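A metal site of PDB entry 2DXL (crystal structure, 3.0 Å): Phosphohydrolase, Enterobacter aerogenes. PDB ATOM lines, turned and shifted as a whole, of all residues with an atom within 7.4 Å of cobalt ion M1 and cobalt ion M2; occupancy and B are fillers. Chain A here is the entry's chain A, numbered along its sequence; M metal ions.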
ATOM      1  N   SER A   7      32.352   3.888  -5.727  1.00  0.00           N
ATOM      2  CA  SER A   7      31.815   4.246  -4.437  1.00  0.00           C
ATOM      3  C   SER A   7      31.421   3.027  -3.654  1.00  0.00           C
ATOM      4  O   SER A   7      31.196   1.949  -4.235  1.00  0.00           O
ATOM      5  CB  SER A   7      30.587   5.138  -4.615  1.00  0.00           C
ATOM      6  OG  SER A   7      30.046   5.523  -3.351  1.00  0.00           O
ATOM      7  N   ASP A   8      31.340   3.190  -2.330  1.00  0.00           N
ATOM      8  CA  ASP A   8      30.706   2.210  -1.485  1.00  0.00           C
ATOM      9  C   ASP A   8      31.282   0.827  -1.654  1.00  0.00           C
ATOM     10  O   ASP A   8      30.552  -0.121  -1.923  1.00  0.00           O
ATOM     11  CB  ASP A   8      29.216   2.196  -1.786  1.00  0.00           C
ATOM     12  CG  ASP A   8      28.476   3.287  -1.069  1.00  0.00           C
ATOM     13  OD1 ASP A   8      28.264   3.108   0.167  1.00  0.00           O
ATOM     14  OD2 ASP A   8      28.137   4.306  -1.730  1.00  0.00           O
ATOM     15  N   THR A   9      32.602   0.732  -1.497  1.00  0.00           N
ATOM     16  CA  THR A   9      33.334  -0.517  -1.626  1.00  0.00           C
ATOM     17  C   THR A   9      33.046  -1.493  -0.493  1.00  0.00           C
ATOM     18  O   THR A   9      33.074  -2.700  -0.694  1.00  0.00           O
ATOM     19  CB  THR A   9      34.818  -0.236  -1.644  1.00  0.00           C
ATOM     20  OG1 THR A   9      35.142   0.546  -0.491  1.00  0.00           O
ATOM     21  CG2 THR A   9      35.173   0.531  -2.874  1.00  0.00           C
ATOM     22  N   HIS A  10      32.766  -0.951   0.694  1.00  0.00           N
ATOM     23  CA  HIS A  10      32.357  -1.726   1.885  1.00  0.00           C
ATOM     24  C   HIS A  10      33.290  -2.887   2.259  1.00  0.00           C
ATOM     25  O   HIS A  10      32.805  -3.996   2.531  1.00  0.00           O
ATOM     26  CB  HIS A  10      30.920  -2.234   1.735  1.00  0.00           C
ATOM     27  CG  HIS A  10      29.868  -1.196   1.990  1.00  0.00           C
ATOM     28  ND1 HIS A  10      29.126  -1.149   3.150  1.00  0.00           N
ATOM     29  CD2 HIS A  10      29.438  -0.160   1.228  1.00  0.00           C
ATOM     30  CE1 HIS A  10      28.283  -0.133   3.087  1.00  0.00           C
ATOM     31  NE2 HIS A  10      28.451   0.487   1.936  1.00  0.00           N
ATOM     32  N   SER A  48      34.018   7.651  -3.325  1.00  0.00           N
ATOM     33  CA  SER A  48      33.160   8.533  -2.515  1.00  0.00           C
ATOM     34  C   SER A  48      32.512   7.820  -1.325  1.00  0.00           C
ATOM     35  O   SER A  48      31.445   8.197  -0.857  1.00  0.00           O
ATOM     36  CB  SER A  48      32.065   9.109  -3.406  1.00  0.00           C
ATOM     37  OG  SER A  48      31.324   8.049  -3.998  1.00  0.00           O
ATOM     38  N   GLY A  49      33.157   6.772  -0.836  1.00  0.00           N
ATOM     39  CA  GLY A  49      32.365   5.634  -0.393  1.00  0.00           C
ATOM     40  C   GLY A  49      32.216   5.475   1.078  1.00  0.00           C
ATOM     41  O   GLY A  49      32.656   6.317   1.867  1.00  0.00           O
ATOM     42  N   ASP A  50      31.525   4.404   1.420  1.00  0.00           N
ATOM     43  CA  ASP A  50      31.702   3.785   2.698  1.00  0.00           C
ATOM     44  C   ASP A  50      32.843   2.837   2.356  1.00  0.00           C
ATOM     45  O   ASP A  50      32.583   1.723   1.885  1.00  0.00           O
ATOM     46  CB  ASP A  50      30.457   3.001   3.054  1.00  0.00           C
ATOM     47  CG  ASP A  50      29.287   3.873   3.406  1.00  0.00           C
ATOM     48  OD1 ASP A  50      29.424   4.787   4.246  1.00  0.00           O
ATOM     49  OD2 ASP A  50      28.202   3.623   2.868  1.00  0.00           O
ATOM     50  N   ILE A  51      34.088   3.292   2.528  1.00  0.00           N
ATOM     51  CA  ILE A  51      35.241   2.510   2.072  1.00  0.00           C
ATOM     52  C   ILE A  51      35.252   1.136   2.768  1.00  0.00           C
ATOM     53  O   ILE A  51      35.505   0.132   2.106  1.00  0.00           O
ATOM     54  CB  ILE A  51      36.630   3.255   2.193  1.00  0.00           C
ATOM     55  CG1 ILE A  51      36.921   4.144   0.986  1.00  0.00           C
ATOM     56  CG2 ILE A  51      37.775   2.284   2.103  1.00  0.00           C
ATOM     57  CD1 ILE A  51      36.161   5.382   0.924  1.00  0.00           C
ATOM     58  N   VAL A  52      34.952   1.106   4.069  1.00  0.00           N
ATOM     59  CA  VAL A  52      34.839  -0.167   4.824  1.00  0.00           C
ATOM     60  C   VAL A  52      33.429  -0.352   5.382  1.00  0.00           C
ATOM     61  O   VAL A  52      32.665   0.602   5.464  1.00  0.00           O
ATOM     62  CB  VAL A  52      35.860  -0.279   6.001  1.00  0.00           C
ATOM     63  CG1 VAL A  52      37.293  -0.074   5.503  1.00  0.00           C
ATOM     64  CG2 VAL A  52      35.523   0.681   7.121  1.00  0.00           C
ATOM     65  N   ASN A  53      33.076  -1.564   5.793  1.00  0.00           N
ATOM     66  CA  ASN A  53      31.709  -1.837   6.228  1.00  0.00           C
ATOM     67  C   ASN A  53      31.416  -1.563   7.705  1.00  0.00           C
ATOM     68  O   ASN A  53      30.349  -1.079   8.041  1.00  0.00           O
ATOM     69  CB  ASN A  53      31.289  -3.255   5.869  1.00  0.00           C
ATOM     70  CG  ASN A  53      29.819  -3.524   6.136  1.00  0.00           C
ATOM     71  OD1 ASN A  53      29.472  -4.315   7.019  1.00  0.00           O
ATOM     72  ND2 ASN A  53      28.952  -2.857   5.392  1.00  0.00           N
ATOM     73  N   GLY A  79      32.353   7.643   4.368  1.00  0.00           N
ATOM     74  CA  GLY A  79      30.904   7.569   4.478  1.00  0.00           C
ATOM     75  C   GLY A  79      30.513   7.218   5.907  1.00  0.00           C
ATOM     76  O   GLY A  79      31.371   7.035   6.765  1.00  0.00           O
ATOM     77  N   ASN A  80      29.208   7.134   6.157  1.00  0.00           N
ATOM     78  CA  ASN A  80      28.698   6.774   7.479  1.00  0.00           C
ATOM     79  C   ASN A  80      29.174   5.408   8.002  1.00  0.00           C
ATOM     80  O   ASN A  80      29.152   5.168   9.209  1.00  0.00           O
ATOM     81  CB  ASN A  80      27.162   6.847   7.493  1.00  0.00           C
ATOM     82  CG  ASN A  80      26.527   5.854   6.545  1.00  0.00           C
ATOM     83  OD1 ASN A  80      26.832   5.808   5.342  1.00  0.00           O
ATOM     84  ND2 ASN A  80      25.626   5.028   7.088  1.00  0.00           N
ATOM     85  N   HIS A  81      29.613   4.521   7.103  1.00  0.00           N
ATOM     86  CA  HIS A  81      30.168   3.236   7.504  1.00  0.00           C
ATOM     87  C   HIS A  81      31.637   3.320   7.906  1.00  0.00           C
ATOM     88  O   HIS A  81      32.208   2.350   8.400  1.00  0.00           O
ATOM     89  CB  HIS A  81      29.989   2.193   6.420  1.00  0.00           C
ATOM     90  CG  HIS A  81      28.622   1.592   6.395  1.00  0.00           C
ATOM     91  ND1 HIS A  81      27.542   2.212   5.793  1.00  0.00           N
ATOM     92  CD2 HIS A  81      28.145   0.447   6.944  1.00  0.00           C
ATOM     93  CE1 HIS A  81      26.469   1.473   5.960  1.00  0.00           C
ATOM     94  NE2 HIS A  81      26.803   0.394   6.649  1.00  0.00           N
ATOM     95  N   ASP A  82      32.229   4.487   7.719  1.00  0.00           N
ATOM     96  CA  ASP A  82      33.623   4.693   8.012  1.00  0.00           C
ATOM     97  C   ASP A  82      33.844   5.240   9.416  1.00  0.00           C
ATOM     98  O   ASP A  82      32.913   5.773  10.042  1.00  0.00           O
ATOM     99  CB  ASP A  82      34.213   5.649   6.982  1.00  0.00           C
ATOM    100  CG  ASP A  82      34.612   4.941   5.721  1.00  0.00           C
ATOM    101  OD1 ASP A  82      35.546   4.105   5.803  1.00  0.00           O
ATOM    102  OD2 ASP A  82      33.999   5.211   4.663  1.00  0.00           O
ATOM    103  N   SER A 127      23.469   7.303  10.624  1.00  0.00           N
ATOM    104  CA  SER A 127      23.643   7.023   9.201  1.00  0.00           C
ATOM    105  C   SER A 127      23.400   8.289   8.390  1.00  0.00           C
ATOM    106  O   SER A 127      23.869   8.394   7.249  1.00  0.00           O
ATOM    107  CB  SER A 127      22.713   5.892   8.743  1.00  0.00           C
ATOM    108  OG  SER A 127      23.065   4.676   9.371  1.00  0.00           O
ATOM    109  N   HIS A 156      29.692  11.883   0.294  1.00  0.00           N
ATOM    110  CA  HIS A 156      29.055  10.581   0.387  1.00  0.00           C
ATOM    111  C   HIS A 156      27.525  10.676   0.346  1.00  0.00           C
ATOM    112  O   HIS A 156      26.888   9.932  -0.411  1.00  0.00           O
ATOM    113  CB  HIS A 156      29.517   9.829   1.637  1.00  0.00           C
ATOM    114  CG  HIS A 156      28.904   8.468   1.801  1.00  0.00           C
ATOM    115  ND1 HIS A 156      29.134   7.443   0.918  1.00  0.00           N
ATOM    116  CD2 HIS A 156      28.071   7.972   2.743  1.00  0.00           C
ATOM    117  CE1 HIS A 156      28.475   6.368   1.316  1.00  0.00           C
ATOM    118  NE2 HIS A 156      27.823   6.659   2.422  1.00  0.00           N
ATOM    119  N   HIS A 157      26.964  11.589   1.132  1.00  0.00           N
ATOM    120  CA  HIS A 157      25.515  11.655   1.276  1.00  0.00           C
ATOM    121  C   HIS A 157      24.902  12.585   0.246  1.00  0.00           C
ATOM    122  O   HIS A 157      25.413  13.684   0.027  1.00  0.00           O
ATOM    123  CB  HIS A 157      25.134  12.148   2.669  1.00  0.00           C
ATOM    124  CG  HIS A 157      25.448  11.178   3.767  1.00  0.00           C
ATOM    125  ND1 HIS A 157      26.695  11.069   4.339  1.00  0.00           N
ATOM    126  CD2 HIS A 157      24.661  10.291   4.424  1.00  0.00           C
ATOM    127  CE1 HIS A 157      26.659  10.153   5.288  1.00  0.00           C
ATOM    128  NE2 HIS A 157      25.440   9.666   5.366  1.00  0.00           N
ATOM    129  N   MET A 167      16.394   5.377   1.451  1.00  0.00           N
ATOM    130  CA  MET A 167      17.592   6.213   1.489  1.00  0.00           C
ATOM    131  C   MET A 167      17.412   7.677   1.900  1.00  0.00           C
ATOM    132  O   MET A 167      18.378   8.342   2.295  1.00  0.00           O
ATOM    133  CB  MET A 167      18.317   6.112   0.147  1.00  0.00           C
ATOM    134  CG  MET A 167      19.043   4.804  -0.073  1.00  0.00           C
ATOM    135  SD  MET A 167      20.144   4.437   1.308  1.00  0.00           S
ATOM    136  CE  MET A 167      19.166   3.280   2.244  1.00  0.00           C
ATOM    137  N   ILE A 170      17.887   8.915   5.561  1.00  0.00           N
ATOM    138  CA  ILE A 170      19.314   8.945   5.890  1.00  0.00           C
ATOM    139  C   ILE A 170      20.176   9.701   4.858  1.00  0.00           C
ATOM    140  O   ILE A 170      21.369   9.433   4.712  1.00  0.00           O
ATOM    141  CB  ILE A 170      19.854   7.532   6.217  1.00  0.00           C
ATOM    142  CG1 ILE A 170      19.600   6.538   5.077  1.00  0.00           C
ATOM    143  CG2 ILE A 170      19.249   7.051   7.542  1.00  0.00           C
ATOM    144  CD1 ILE A 170      20.330   5.196   5.207  1.00  0.00           C
ATOM    145  N   GLY A 194      27.759   9.032  -3.051  1.00  0.00           N
ATOM    146  CA  GLY A 194      27.600   7.609  -2.798  1.00  0.00           C
ATOM    147  C   GLY A 194      26.298   7.340  -2.071  1.00  0.00           C
ATOM    148  O   GLY A 194      25.239   7.868  -2.458  1.00  0.00           O
ATOM    149  N   HIS A 195      26.367   6.512  -1.030  1.00  0.00           N
ATOM    150  CA  HIS A 195      25.257   6.241  -0.113  1.00  0.00           C
ATOM    151  C   HIS A 195      24.096   5.430  -0.689  1.00  0.00           C
ATOM    152  O   HIS A 195      23.710   4.431  -0.104  1.00  0.00           O
ATOM    153  CB  HIS A 195      24.736   7.540   0.507  1.00  0.00           C
ATOM    154  CG  HIS A 195      24.090   7.364   1.850  1.00  0.00           C
ATOM    155  ND1 HIS A 195      24.739   6.785   2.921  1.00  0.00           N
ATOM    156  CD2 HIS A 195      22.860   7.710   2.306  1.00  0.00           C
ATOM    157  CE1 HIS A 195      23.945   6.782   3.972  1.00  0.00           C
ATOM    158  NE2 HIS A 195      22.798   7.335   3.623  1.00  0.00           N
ATOM    159  N   ASN A 196      23.556   5.850  -1.826  1.00  0.00           N
ATOM    160  CA  ASN A 196      22.340   5.239  -2.375  1.00  0.00           C
ATOM    161  C   ASN A 196      22.511   3.888  -3.073  1.00  0.00           C
ATOM    162  O   ASN A 196      21.523   3.191  -3.311  1.00  0.00           O
ATOM    163  CB  ASN A 196      21.619   6.225  -3.291  1.00  0.00           C
ATOM    164  CG  ASN A 196      20.571   7.049  -2.565  1.00  0.00           C
ATOM    165  OD1 ASN A 196      20.794   7.549  -1.455  1.00  0.00           O
ATOM    166  ND2 ASN A 196      19.411   7.196  -3.186  1.00  0.00           N
ATOM    167  N   HIS A 197      23.747   3.528  -3.385  1.00  0.00           N
ATOM    168  CA  HIS A 197      24.074   2.313  -4.163  1.00  0.00           C
ATOM    169  C   HIS A 197      23.159   2.177  -5.385  1.00  0.00           C
ATOM    170  O   HIS A 197      22.475   1.156  -5.562  1.00  0.00           O
ATOM    171  CB  HIS A 197      23.959   1.050  -3.323  1.00  0.00           C
ATOM    172  CG  HIS A 197      24.938   0.980  -2.190  1.00  0.00           C
ATOM    173  ND1 HIS A 197      25.816  -0.080  -2.044  1.00  0.00           N
ATOM    174  CD2 HIS A 197      25.161   1.808  -1.146  1.00  0.00           C
ATOM    175  CE1 HIS A 197      26.541   0.115  -0.953  1.00  0.00           C
ATOM    176  NE2 HIS A 197      26.173   1.252  -0.395  1.00  0.00           N
ATOM    177  N   GLY A 214      27.035   1.016  -6.235  1.00  0.00           N
ATOM    178  CA  GLY A 214      28.187   0.543  -5.466  1.00  0.00           C
ATOM    179  C   GLY A 214      29.044  -0.367  -6.336  1.00  0.00           C
ATOM    180  O   GLY A 214      28.599  -0.823  -7.395  1.00  0.00           O
ATOM    181  N   HIS A 217      27.465  -4.722  -4.005  1.00  0.00           N
ATOM    182  CA  HIS A 217      26.022  -4.846  -3.898  1.00  0.00           C
ATOM    183  C   HIS A 217      25.317  -3.508  -4.114  1.00  0.00           C
ATOM    184  O   HIS A 217      25.889  -2.439  -3.898  1.00  0.00           O
ATOM    185  CB  HIS A 217      25.675  -5.430  -2.549  1.00  0.00           C
ATOM    186  CG  HIS A 217      26.034  -4.551  -1.397  1.00  0.00           C
ATOM    187  ND1 HIS A 217      27.295  -4.020  -1.240  1.00  0.00           N
ATOM    188  CD2 HIS A 217      25.299  -4.096  -0.355  1.00  0.00           C
ATOM    189  CE1 HIS A 217      27.328  -3.265  -0.159  1.00  0.00           C
ATOM    190  NE2 HIS A 217      26.127  -3.303   0.402  1.00  0.00           N
ATOM    191  N   VAL A 219      21.433  -1.163  -3.869  1.00  0.00           N
ATOM    192  CA  VAL A 219      20.114  -1.062  -3.241  1.00  0.00           C
ATOM    193  C   VAL A 219      19.053  -0.451  -4.178  1.00  0.00           C
ATOM    194  O   VAL A 219      19.274   0.609  -4.778  1.00  0.00           O
ATOM    195  CB  VAL A 219      20.126  -0.463  -1.760  1.00  0.00           C
ATOM    196  CG1 VAL A 219      21.481   0.086  -1.367  1.00  0.00           C
ATOM    197  CG2 VAL A 219      19.021   0.568  -1.545  1.00  0.00           C
HETATM  198 CO    CO M   1      26.412   5.170   3.329  1.00  0.00          CO
HETATM  199 CO    CO M   2      26.982   2.157   1.392  1.00  0.00          CO
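Within 4 Å of cobalt ion M2: Asp 8, His 10, Asp 50 and His 197.
Cobalt ion M2 is bound by the side-chain carboxylate of Asp 8 (2.0 Å), a ring nitrogen (NE2) of His 197 (2.2 Å), a ring nitrogen (NE2) of His 10 (2.3 Å) and the side-chain carboxylate of Asp 50 (2.4 Å).
Cobalt ion M1 is bound by OD1 of Asn 80, at 2.2 Å. Cobalt ion M1 is bound by NE2 of His 156 (2.2 Å). ND1 of His 195 is bound to cobalt ion M1, 2.4 Å away. OD2 of Asp 50 binds cobalt ion M1 (2.4 Å). Cobalt ion M1 has four donor atoms within binding distance.
Within 4 Å of cobalt ion M1: Asp 50, Asn 80, His 156 and His 195. The nearest printed residue that does not touch cobalt ion M1 is His 81 (4.01 Å).
The side-chain carboxylate (OD2) of Asp 8 is in hydrogen-bond range of the backbone NH (N) of His 195, 2.9 Å away. The side-chain carboxylate (OD2) of Asp 8 sits at hydrogen-bond distance from the side-chain hydroxyl (OG) of Ser 7 (2.8 Å). O of His 217 lies within hydrogen-bond range of ND1 of His 197 (3.0 Å). The backbone carbonyl oxygen (O) of His 197 is in hydrogen-bond range of the backbone NH (N) of Val 219, at 3.1 Å. The backbone carbonyl oxygen of His 156 is in hydrogen-bond range of the backbone NH of Gly 194, at 2.9 Å. A ring nitrogen (ND1) of His 156 sits at hydrogen-bond distance from the backbone carbonyl oxygen of Ser 48, 3.0 Å away. A ring nitrogen (ND1) of His 10 sits at hydrogen-bond distance from the side-chain amide nitrogen (ND2) of Asn 53, at 2.8 Å. The backbone carbonyl oxygen of Ile 170 lies within hydrogen-bond range of a ring nitrogen (NE2) of His 195, at 2.8 Å.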
